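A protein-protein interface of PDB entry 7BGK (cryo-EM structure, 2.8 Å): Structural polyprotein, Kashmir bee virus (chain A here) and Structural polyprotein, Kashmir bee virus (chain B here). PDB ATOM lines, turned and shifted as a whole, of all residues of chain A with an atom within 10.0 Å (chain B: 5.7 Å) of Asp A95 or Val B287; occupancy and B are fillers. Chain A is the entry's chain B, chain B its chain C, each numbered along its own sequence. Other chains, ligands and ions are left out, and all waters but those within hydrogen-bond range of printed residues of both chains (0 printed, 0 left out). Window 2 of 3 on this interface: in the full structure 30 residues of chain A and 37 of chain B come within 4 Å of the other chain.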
ATOM      1  N   SER A  90      30.158  25.395   0.815  1.00  0.00           N
ATOM      2  CA  SER A  90      31.154  25.135  -0.212  1.00  0.00           C
ATOM      3  C   SER A  90      30.742  25.695  -1.566  1.00  0.00           C
ATOM      4  O   SER A  90      29.579  25.604  -1.966  1.00  0.00           O
ATOM      5  CB  SER A  90      31.409  23.634  -0.314  1.00  0.00           C
ATOM      6  OG  SER A  90      32.337  23.329  -1.331  1.00  0.00           O
ATOM      7  N   TYR A  92      31.403  24.700  -4.635  1.00  0.00           N
ATOM      8  CA  TYR A  92      30.894  23.682  -5.537  1.00  0.00           C
ATOM      9  C   TYR A  92      30.592  22.402  -4.774  1.00  0.00           C
ATOM     10  O   TYR A  92      31.075  22.179  -3.663  1.00  0.00           O
ATOM     11  CB  TYR A  92      31.888  23.375  -6.662  1.00  0.00           C
ATOM     12  CG  TYR A  92      32.408  24.584  -7.391  1.00  0.00           C
ATOM     13  CD1 TYR A  92      31.725  25.116  -8.469  1.00  0.00           C
ATOM     14  CD2 TYR A  92      33.586  25.193  -7.004  1.00  0.00           C
ATOM     15  CE1 TYR A  92      32.199  26.213  -9.132  1.00  0.00           C
ATOM     16  CE2 TYR A  92      34.067  26.293  -7.665  1.00  0.00           C
ATOM     17  CZ  TYR A  92      33.368  26.801  -8.729  1.00  0.00           C
ATOM     18  OH  TYR A  92      33.846  27.903  -9.392  1.00  0.00           O
ATOM     19  N   VAL A  93      29.776  21.563  -5.401  1.00  0.00           N
ATOM     20  CA  VAL A  93      29.504  20.208  -4.942  1.00  0.00           C
ATOM     21  C   VAL A  93      29.586  19.325  -6.176  1.00  0.00           C
ATOM     22  O   VAL A  93      28.668  19.316  -7.003  1.00  0.00           O
ATOM     23  CB  VAL A  93      28.145  20.076  -4.253  1.00  0.00           C
ATOM     24  CG1 VAL A  93      27.832  18.636  -3.966  1.00  0.00           C
ATOM     25  CG2 VAL A  93      28.118  20.877  -2.992  1.00  0.00           C
ATOM     26  N   LEU A  94      30.683  18.591  -6.312  1.00  0.00           N
ATOM     27  CA  LEU A  94      30.892  17.758  -7.482  1.00  0.00           C
ATOM     28  C   LEU A  94      30.377  16.345  -7.295  1.00  0.00           C
ATOM     29  O   LEU A  94      30.072  15.676  -8.287  1.00  0.00           O
ATOM     30  CB  LEU A  94      32.381  17.707  -7.829  1.00  0.00           C
ATOM     31  CG  LEU A  94      33.092  19.051  -7.943  1.00  0.00           C
ATOM     32  CD1 LEU A  94      34.564  18.852  -8.141  1.00  0.00           C
ATOM     33  CD2 LEU A  94      32.526  19.855  -9.080  1.00  0.00           C
ATOM     34  N   ASP A  95      30.260  15.881  -6.054  1.00  0.00           N
ATOM     35  CA  ASP A  95      29.833  14.522  -5.777  1.00  0.00           C
ATOM     36  C   ASP A  95      28.946  14.530  -4.541  1.00  0.00           C
ATOM     37  O   ASP A  95      28.965  15.470  -3.745  1.00  0.00           O
ATOM     38  CB  ASP A  95      31.034  13.599  -5.565  1.00  0.00           C
ATOM     39  CG  ASP A  95      31.970  13.533  -6.756  1.00  0.00           C
ATOM     40  OD1 ASP A  95      31.491  13.632  -7.905  1.00  0.00           O
ATOM     41  OD2 ASP A  95      33.192  13.399  -6.542  1.00  0.00           O
ATOM     42  N   ARG A  96      28.163  13.465  -4.389  1.00  0.00           N
ATOM     43  CA  ARG A  96      27.272  13.336  -3.244  1.00  0.00           C
ATOM     44  C   ARG A  96      27.982  12.855  -1.988  1.00  0.00           C
ATOM     45  O   ARG A  96      27.454  13.045  -0.889  1.00  0.00           O
ATOM     46  CB  ARG A  96      26.123  12.386  -3.568  1.00  0.00           C
ATOM     47  CG  ARG A  96      25.228  12.862  -4.687  1.00  0.00           C
ATOM     48  CD  ARG A  96      24.108  11.889  -4.950  1.00  0.00           C
ATOM     49  NE  ARG A  96      23.842  11.748  -6.374  1.00  0.00           N
ATOM     50  CZ  ARG A  96      23.248  10.694  -6.922  1.00  0.00           C
ATOM     51  NH1 ARG A  96      22.852   9.683  -6.166  1.00  0.00           N
ATOM     52  NH2 ARG A  96      23.052  10.651  -8.230  1.00  0.00           N
ATOM     53  N   THR A  97      29.151  12.226  -2.117  1.00  0.00           N
ATOM     54  CA  THR A  97      29.962  11.921  -0.946  1.00  0.00           C
ATOM     55  C   THR A  97      30.589  13.161  -0.327  1.00  0.00           C
ATOM     56  O   THR A  97      31.304  13.039   0.673  1.00  0.00           O
ATOM     57  CB  THR A  97      31.063  10.929  -1.313  1.00  0.00           C
ATOM     58  OG1 THR A  97      31.884  11.482  -2.348  1.00  0.00           O
ATOM     59  CG2 THR A  97      30.466   9.633  -1.803  1.00  0.00           C
ATOM     60  N   ASN A  98      30.338  14.335  -0.891  1.00  0.00           N
ATOM     61  CA  ASN A  98      30.979  15.580  -0.498  1.00  0.00           C
ATOM     62  C   ASN A  98      29.943  16.696  -0.519  1.00  0.00           C
ATOM     63  O   ASN A  98      30.153  17.718  -1.183  1.00  0.00           O
ATOM     64  CB  ASN A  98      32.141  15.926  -1.427  1.00  0.00           C
ATOM     65  CG  ASN A  98      33.018  17.027  -0.868  1.00  0.00           C
ATOM     66  OD1 ASN A  98      32.645  17.699   0.094  1.00  0.00           O
ATOM     67  ND2 ASN A  98      34.170  17.246  -1.489  1.00  0.00           N
ATOM     68  N   PRO A  99      28.825  16.548   0.177  1.00  0.00           N
ATOM     69  CA  PRO A  99      27.729  17.504   0.038  1.00  0.00           C
ATOM     70  C   PRO A  99      27.942  18.723   0.928  1.00  0.00           C
ATOM     71  O   PRO A  99      28.944  18.855   1.624  1.00  0.00           O
ATOM     72  CB  PRO A  99      26.518  16.691   0.476  1.00  0.00           C
ATOM     73  CG  PRO A  99      27.047  15.755   1.483  1.00  0.00           C
ATOM     74  CD  PRO A  99      28.501  15.506   1.165  1.00  0.00           C
ATOM     75  N   GLN A 100      26.967  19.624   0.889  1.00  0.00           N
ATOM     76  CA  GLN A 100      27.027  20.814   1.718  1.00  0.00           C
ATOM     77  C   GLN A 100      26.762  20.458   3.171  1.00  0.00           C
ATOM     78  O   GLN A 100      25.886  19.649   3.484  1.00  0.00           O
ATOM     79  CB  GLN A 100      26.016  21.851   1.240  1.00  0.00           C
ATOM     80  CG  GLN A 100      26.326  22.457  -0.100  1.00  0.00           C
ATOM     81  CD  GLN A 100      27.538  23.340  -0.080  1.00  0.00           C
ATOM     82  OE1 GLN A 100      28.245  23.427   0.921  1.00  0.00           O
ATOM     83  NE2 GLN A 100      27.792  24.005  -1.190  1.00  0.00           N
ATOM     84  N   LYS A 101      27.533  21.071   4.062  1.00  0.00           N
ATOM     85  CA  LYS A 101      27.418  20.815   5.485  1.00  0.00           C
ATOM     86  C   LYS A 101      26.485  21.832   6.119  1.00  0.00           C
ATOM     87  O   LYS A 101      26.451  22.998   5.717  1.00  0.00           O
ATOM     88  CB  LYS A 101      28.790  20.871   6.153  1.00  0.00           C
ATOM     89  CG  LYS A 101      29.845  20.037   5.473  1.00  0.00           C
ATOM     90  CD  LYS A 101      29.606  18.565   5.687  1.00  0.00           C
ATOM     91  CE  LYS A 101      30.752  17.736   5.154  1.00  0.00           C
ATOM     92  NZ  LYS A 101      32.047  18.094   5.791  1.00  0.00           N
ATOM     93  N   PRO A 161      18.010  14.166  -6.396  1.00  0.00           N
ATOM     94  CA  PRO A 161      19.168  14.753  -5.704  1.00  0.00           C
ATOM     95  C   PRO A 161      19.687  16.023  -6.347  1.00  0.00           C
ATOM     96  O   PRO A 161      20.047  16.968  -5.634  1.00  0.00           O
ATOM     97  CB  PRO A 161      20.206  13.625  -5.750  1.00  0.00           C
ATOM     98  CG  PRO A 161      19.774  12.736  -6.846  1.00  0.00           C
ATOM     99  CD  PRO A 161      18.290  12.806  -6.881  1.00  0.00           C
ATOM    100  N   GLU A 162      19.746  16.076  -7.675  1.00  0.00           N
ATOM    101  CA  GLU A 162      20.218  17.281  -8.345  1.00  0.00           C
ATOM    102  C   GLU A 162      19.384  18.502  -7.991  1.00  0.00           C
ATOM    103  O   GLU A 162      19.864  19.630  -8.145  1.00  0.00           O
ATOM    104  CB  GLU A 162      20.218  17.069  -9.856  1.00  0.00           C
ATOM    105  CG  GLU A 162      18.898  16.589 -10.429  1.00  0.00           C
ATOM    106  CD  GLU A 162      18.837  15.088 -10.614  1.00  0.00           C
ATOM    107  OE1 GLU A 162      19.653  14.370 -10.000  1.00  0.00           O
ATOM    108  OE2 GLU A 162      17.966  14.624 -11.376  1.00  0.00           O
ATOM    109  N   ILE A 166      20.879  20.502  -0.466  1.00  0.00           N
ATOM    110  CA  ILE A 166      22.058  19.657  -0.411  1.00  0.00           C
ATOM    111  C   ILE A 166      22.350  19.190  -1.827  1.00  0.00           C
ATOM    112  O   ILE A 166      21.432  18.958  -2.623  1.00  0.00           O
ATOM    113  CB  ILE A 166      21.823  18.477   0.547  1.00  0.00           C
ATOM    114  CG1 ILE A 166      21.347  18.968   1.912  1.00  0.00           C
ATOM    115  CG2 ILE A 166      23.067  17.662   0.723  1.00  0.00           C
ATOM    116  CD1 ILE A 166      22.249  19.967   2.569  1.00  0.00           C
ATOM    117  N   TYR A 167      23.628  19.066  -2.160  1.00  0.00           N
ATOM    118  CA  TYR A 167      24.084  18.686  -3.491  1.00  0.00           C
ATOM    119  C   TYR A 167      23.980  19.820  -4.502  1.00  0.00           C
ATOM    120  O   TYR A 167      23.893  19.562  -5.705  1.00  0.00           O
ATOM    121  CB  TYR A 167      23.326  17.471  -4.038  1.00  0.00           C
ATOM    122  CG  TYR A 167      23.240  16.305  -3.088  1.00  0.00           C
ATOM    123  CD1 TYR A 167      24.358  15.853  -2.416  1.00  0.00           C
ATOM    124  CD2 TYR A 167      22.046  15.645  -2.881  1.00  0.00           C
ATOM    125  CE1 TYR A 167      24.285  14.787  -1.557  1.00  0.00           C
ATOM    126  CE2 TYR A 167      21.963  14.578  -2.023  1.00  0.00           C
ATOM    127  CZ  TYR A 167      23.086  14.152  -1.363  1.00  0.00           C
ATOM    128  OH  TYR A 167      23.011  13.083  -0.503  1.00  0.00           O
ATOM    129  N   THR A 168      23.982  21.070  -4.054  1.00  0.00           N
ATOM    130  CA  THR A 168      24.103  22.221  -4.936  1.00  0.00           C
ATOM    131  C   THR A 168      25.150  23.169  -4.373  1.00  0.00           C
ATOM    132  O   THR A 168      25.747  22.926  -3.321  1.00  0.00           O
ATOM    133  CB  THR A 168      22.769  22.947  -5.151  1.00  0.00           C
ATOM    134  OG1 THR A 168      22.893  23.820  -6.276  1.00  0.00           O
ATOM    135  CG2 THR A 168      22.375  23.764  -3.952  1.00  0.00           C
ATOM    136  N   SER A 169      25.373  24.258  -5.093  1.00  0.00           N
ATOM    137  CA  SER A 169      26.457  25.176  -4.804  1.00  0.00           C
ATOM    138  C   SER A 169      26.057  26.203  -3.752  1.00  0.00           C
ATOM    139  O   SER A 169      24.900  26.311  -3.345  1.00  0.00           O
ATOM    140  CB  SER A 169      26.899  25.896  -6.070  1.00  0.00           C
ATOM    141  OG  SER A 169      25.796  26.309  -6.850  1.00  0.00           O
ATOM    142  N   ARG B 103      35.995  18.927 -12.815  1.00  0.00           N
ATOM    143  CA  ARG B 103      35.898  17.616 -12.192  1.00  0.00           C
ATOM    144  C   ARG B 103      36.624  16.604 -13.067  1.00  0.00           C
ATOM    145  O   ARG B 103      36.218  16.359 -14.208  1.00  0.00           O
ATOM    146  CB  ARG B 103      34.441  17.215 -12.002  1.00  0.00           C
ATOM    147  CG  ARG B 103      34.247  15.832 -11.442  1.00  0.00           C
ATOM    148  CD  ARG B 103      32.793  15.541 -11.249  1.00  0.00           C
ATOM    149  NE  ARG B 103      32.559  14.242 -10.631  1.00  0.00           N
ATOM    150  CZ  ARG B 103      32.560  13.092 -11.291  1.00  0.00           C
ATOM    151  NH1 ARG B 103      32.328  11.964 -10.647  1.00  0.00           N
ATOM    152  NH2 ARG B 103      32.789  13.065 -12.593  1.00  0.00           N
ATOM    153  N   TYR B 282      24.018  19.958 -14.028  1.00  0.00           N
ATOM    154  CA  TYR B 282      24.965  19.002 -13.479  1.00  0.00           C
ATOM    155  C   TYR B 282      24.294  18.191 -12.384  1.00  0.00           C
ATOM    156  O   TYR B 282      23.890  18.743 -11.355  1.00  0.00           O
ATOM    157  CB  TYR B 282      26.193  19.723 -12.937  1.00  0.00           C
ATOM    158  CG  TYR B 282      27.218  18.818 -12.312  1.00  0.00           C
ATOM    159  CD1 TYR B 282      27.993  17.981 -13.091  1.00  0.00           C
ATOM    160  CD2 TYR B 282      27.423  18.812 -10.946  1.00  0.00           C
ATOM    161  CE1 TYR B 282      28.930  17.161 -12.529  1.00  0.00           C
ATOM    162  CE2 TYR B 282      28.357  17.995 -10.379  1.00  0.00           C
ATOM    163  CZ  TYR B 282      29.111  17.172 -11.173  1.00  0.00           C
ATOM    164  OH  TYR B 282      30.048  16.350 -10.606  1.00  0.00           O
ATOM    165  N   PRO B 284      25.157  15.765  -9.652  1.00  0.00           N
ATOM    166  CA  PRO B 284      26.320  15.209  -8.972  1.00  0.00           C
ATOM    167  C   PRO B 284      26.204  13.704  -8.836  1.00  0.00           C
ATOM    168  O   PRO B 284      25.231  13.198  -8.259  1.00  0.00           O
ATOM    169  CB  PRO B 284      26.290  15.898  -7.603  1.00  0.00           C
ATOM    170  CG  PRO B 284      25.547  17.122  -7.818  1.00  0.00           C
ATOM    171  CD  PRO B 284      24.502  16.790  -8.826  1.00  0.00           C
ATOM    172  N   PRO B 285      27.167  12.951  -9.359  1.00  0.00           N
ATOM    173  CA  PRO B 285      27.129  11.500  -9.187  1.00  0.00           C
ATOM    174  C   PRO B 285      27.423  11.104  -7.751  1.00  0.00           C
ATOM    175  O   PRO B 285      27.923  11.890  -6.945  1.00  0.00           O
ATOM    176  CB  PRO B 285      28.215  11.004 -10.142  1.00  0.00           C
ATOM    177  CG  PRO B 285      29.134  12.135 -10.283  1.00  0.00           C
ATOM    178  CD  PRO B 285      28.315  13.370 -10.178  1.00  0.00           C
ATOM    179  N   ALA B 286      27.093   9.852  -7.440  1.00  0.00           N
ATOM    180  CA  ALA B 286      27.252   9.359  -6.078  1.00  0.00           C
ATOM    181  C   ALA B 286      28.710   9.401  -5.643  1.00  0.00           C
ATOM    182  O   ALA B 286      29.072  10.116  -4.703  1.00  0.00           O
ATOM    183  CB  ALA B 286      26.698   7.942  -5.980  1.00  0.00           C
ATOM    184  N   VAL B 287      29.562   8.649  -6.323  1.00  0.00           N
ATOM    185  CA  VAL B 287      30.961   8.536  -5.962  1.00  0.00           C
ATOM    186  C   VAL B 287      31.791   9.352  -6.940  1.00  0.00           C
ATOM    187  O   VAL B 287      31.365   9.667  -8.055  1.00  0.00           O
ATOM    188  CB  VAL B 287      31.431   7.060  -5.939  1.00  0.00           C
ATOM    189  CG1 VAL B 287      32.789   6.926  -5.258  1.00  0.00           C
ATOM    190  CG2 VAL B 287      30.409   6.182  -5.248  1.00  0.00           C
ATOM    191  N   ALA B 288      32.998   9.709  -6.507  1.00  0.00           N
ATOM    192  CA  ALA B 288      33.896  10.485  -7.348  1.00  0.00           C
ATOM    193  C   ALA B 288      34.449   9.656  -8.498  1.00  0.00           C
ATOM    194  O   ALA B 288      34.928  10.229  -9.482  1.00  0.00           O
ATOM    195  CB  ALA B 288      35.036  11.054  -6.508  1.00  0.00           C
ATOM    196  N   ARG B 289      34.402   8.325  -8.395  1.00  0.00           N
ATOM    197  CA  ARG B 289      34.828   7.482  -9.504  1.00  0.00           C
ATOM    198  C   ARG B 289      33.816   7.470 -10.638  1.00  0.00           C
ATOM    199  O   ARG B 289      34.152   7.047 -11.748  1.00  0.00           O
ATOM    200  CB  ARG B 289      35.018   6.032  -9.048  1.00  0.00           C
ATOM    201  CG  ARG B 289      33.708   5.345  -8.624  1.00  0.00           C
ATOM    202  CD  ARG B 289      33.849   3.834  -8.503  1.00  0.00           C
ATOM    203  NE  ARG B 289      32.541   3.177  -8.496  1.00  0.00           N
ATOM    204  CZ  ARG B 289      31.969   2.600  -7.442  1.00  0.00           C
ATOM    205  NH1 ARG B 289      32.569   2.577  -6.259  1.00  0.00           N
ATOM    206  NH2 ARG B 289      30.774   2.040  -7.576  1.00  0.00           N
ATOM    207  N   ASP B 290      32.594   7.921 -10.385  1.00  0.00           N
ATOM    208  CA  ASP B 290      31.531   7.824 -11.371  1.00  0.00           C
ATOM    209  C   ASP B 290      31.667   8.892 -12.444  1.00  0.00           C
ATOM    210  O   ASP B 290      32.011  10.042 -12.161  1.00  0.00           O
ATOM    211  CB  ASP B 290      30.170   7.946 -10.691  1.00  0.00           C
ATOM    212  CG  ASP B 290      29.822   6.732  -9.857  1.00  0.00           C
ATOM    213  OD1 ASP B 290      30.290   5.624 -10.190  1.00  0.00           O
ATOM    214  OD2 ASP B 290      29.068   6.884  -8.873  1.00  0.00           O
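Among the printed residues, merely in contact across the chains: Val A93 with Tyr B282 (3.6 Å), Val A93 with Pro B284 (3.9 Å), Leu A94 with Arg B103 (3.7 Å), Leu A94 with Pro B284 (3.8 Å), Leu A94 with Pro B285 (3.5 Å), Asp A95 with Pro B285 (3.5 Å), Asp A95 with Val B287 (3.97 Å), Asp A95 with Ala B288 (3.0 Å) and Tyr A167 with Pro B284 (3.6 Å).
Hydrophobic or aromatic side chains of chain B that line the printed part of chain A: Tyr B282, Pro B284, Pro B285 and Ala B288. Hydrophobic or aromatic side chains of chain A within 4 Å of the printed part of chain B: Leu A94. Among the printed residues, 15 pairs touch across the chains.
The guanidinium group of Arg B103 lies close to the side-chain hydroxyl of Tyr B282 (3.3 Å). O of Ala B288 sits at hydrogen-bond distance from NH1 of Arg B103 (3.3 Å). The guanidinium group (NH1) of Arg B103 lies within hydrogen-bond range of the backbone carbonyl oxygen (O) of Asp B290 (2.5 Å). The backbone NH of Val B287 lies within hydrogen-bond range of the side-chain carboxylate of Asp B290.
The guanidinium group (NE) of Arg B103 is in salt-bridge range of the side-chain carboxylate (OD1) of Asp A95, 3.0 Å away. The side-chain hydroxyl (OH) of Tyr B282 is in hydrogen-bond range of the backbone carbonyl oxygen (O) of Leu A94. The guanidinium group of Arg A96 sits at hydrogen-bond distance from the backbone carbonyl oxygen of Pro B284 (2.8 Å). The backbone carbonyl oxygen of Pro B285 is in hydrogen-bond range of the backbone NH of Arg A96 (3.0 Å). The backbone NH (N) of Arg A96 lies within hydrogen-bond range of the backbone carbonyl oxygen (O) of Ala B286 (3.5 Å). N of Thr A97 lies close to O of Ala B286.
Of chain B, only Arg B103, Pro B285, Val B287 and Ala B288 come within 4 Å of Asp A95. Printed residues of chain A within 4 Å of Val B287: Asp A95. Pro B285 touches three residues of chain A. Of the printed residues of chain A, Ala B286 touches Arg A96 and Thr A97. Ala B288 touches just one residue of chain A: Asp A95. No residue of chain A comes within 4 Å of Arg B289. Printed residues of chain B within 4 Å of Val A93: Tyr B282 and Pro B284. Of the printed residues of chain B, Arg A96 touches Pro B284, Pro B285 and Ala B286. Glu A162 touches none of the printed residues of chain B. Ile A166 touches none of the printed residues of chain B. The nearest printed residue of chain B that does not touch Asp A95 is Ala B286 (4.1 Å).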
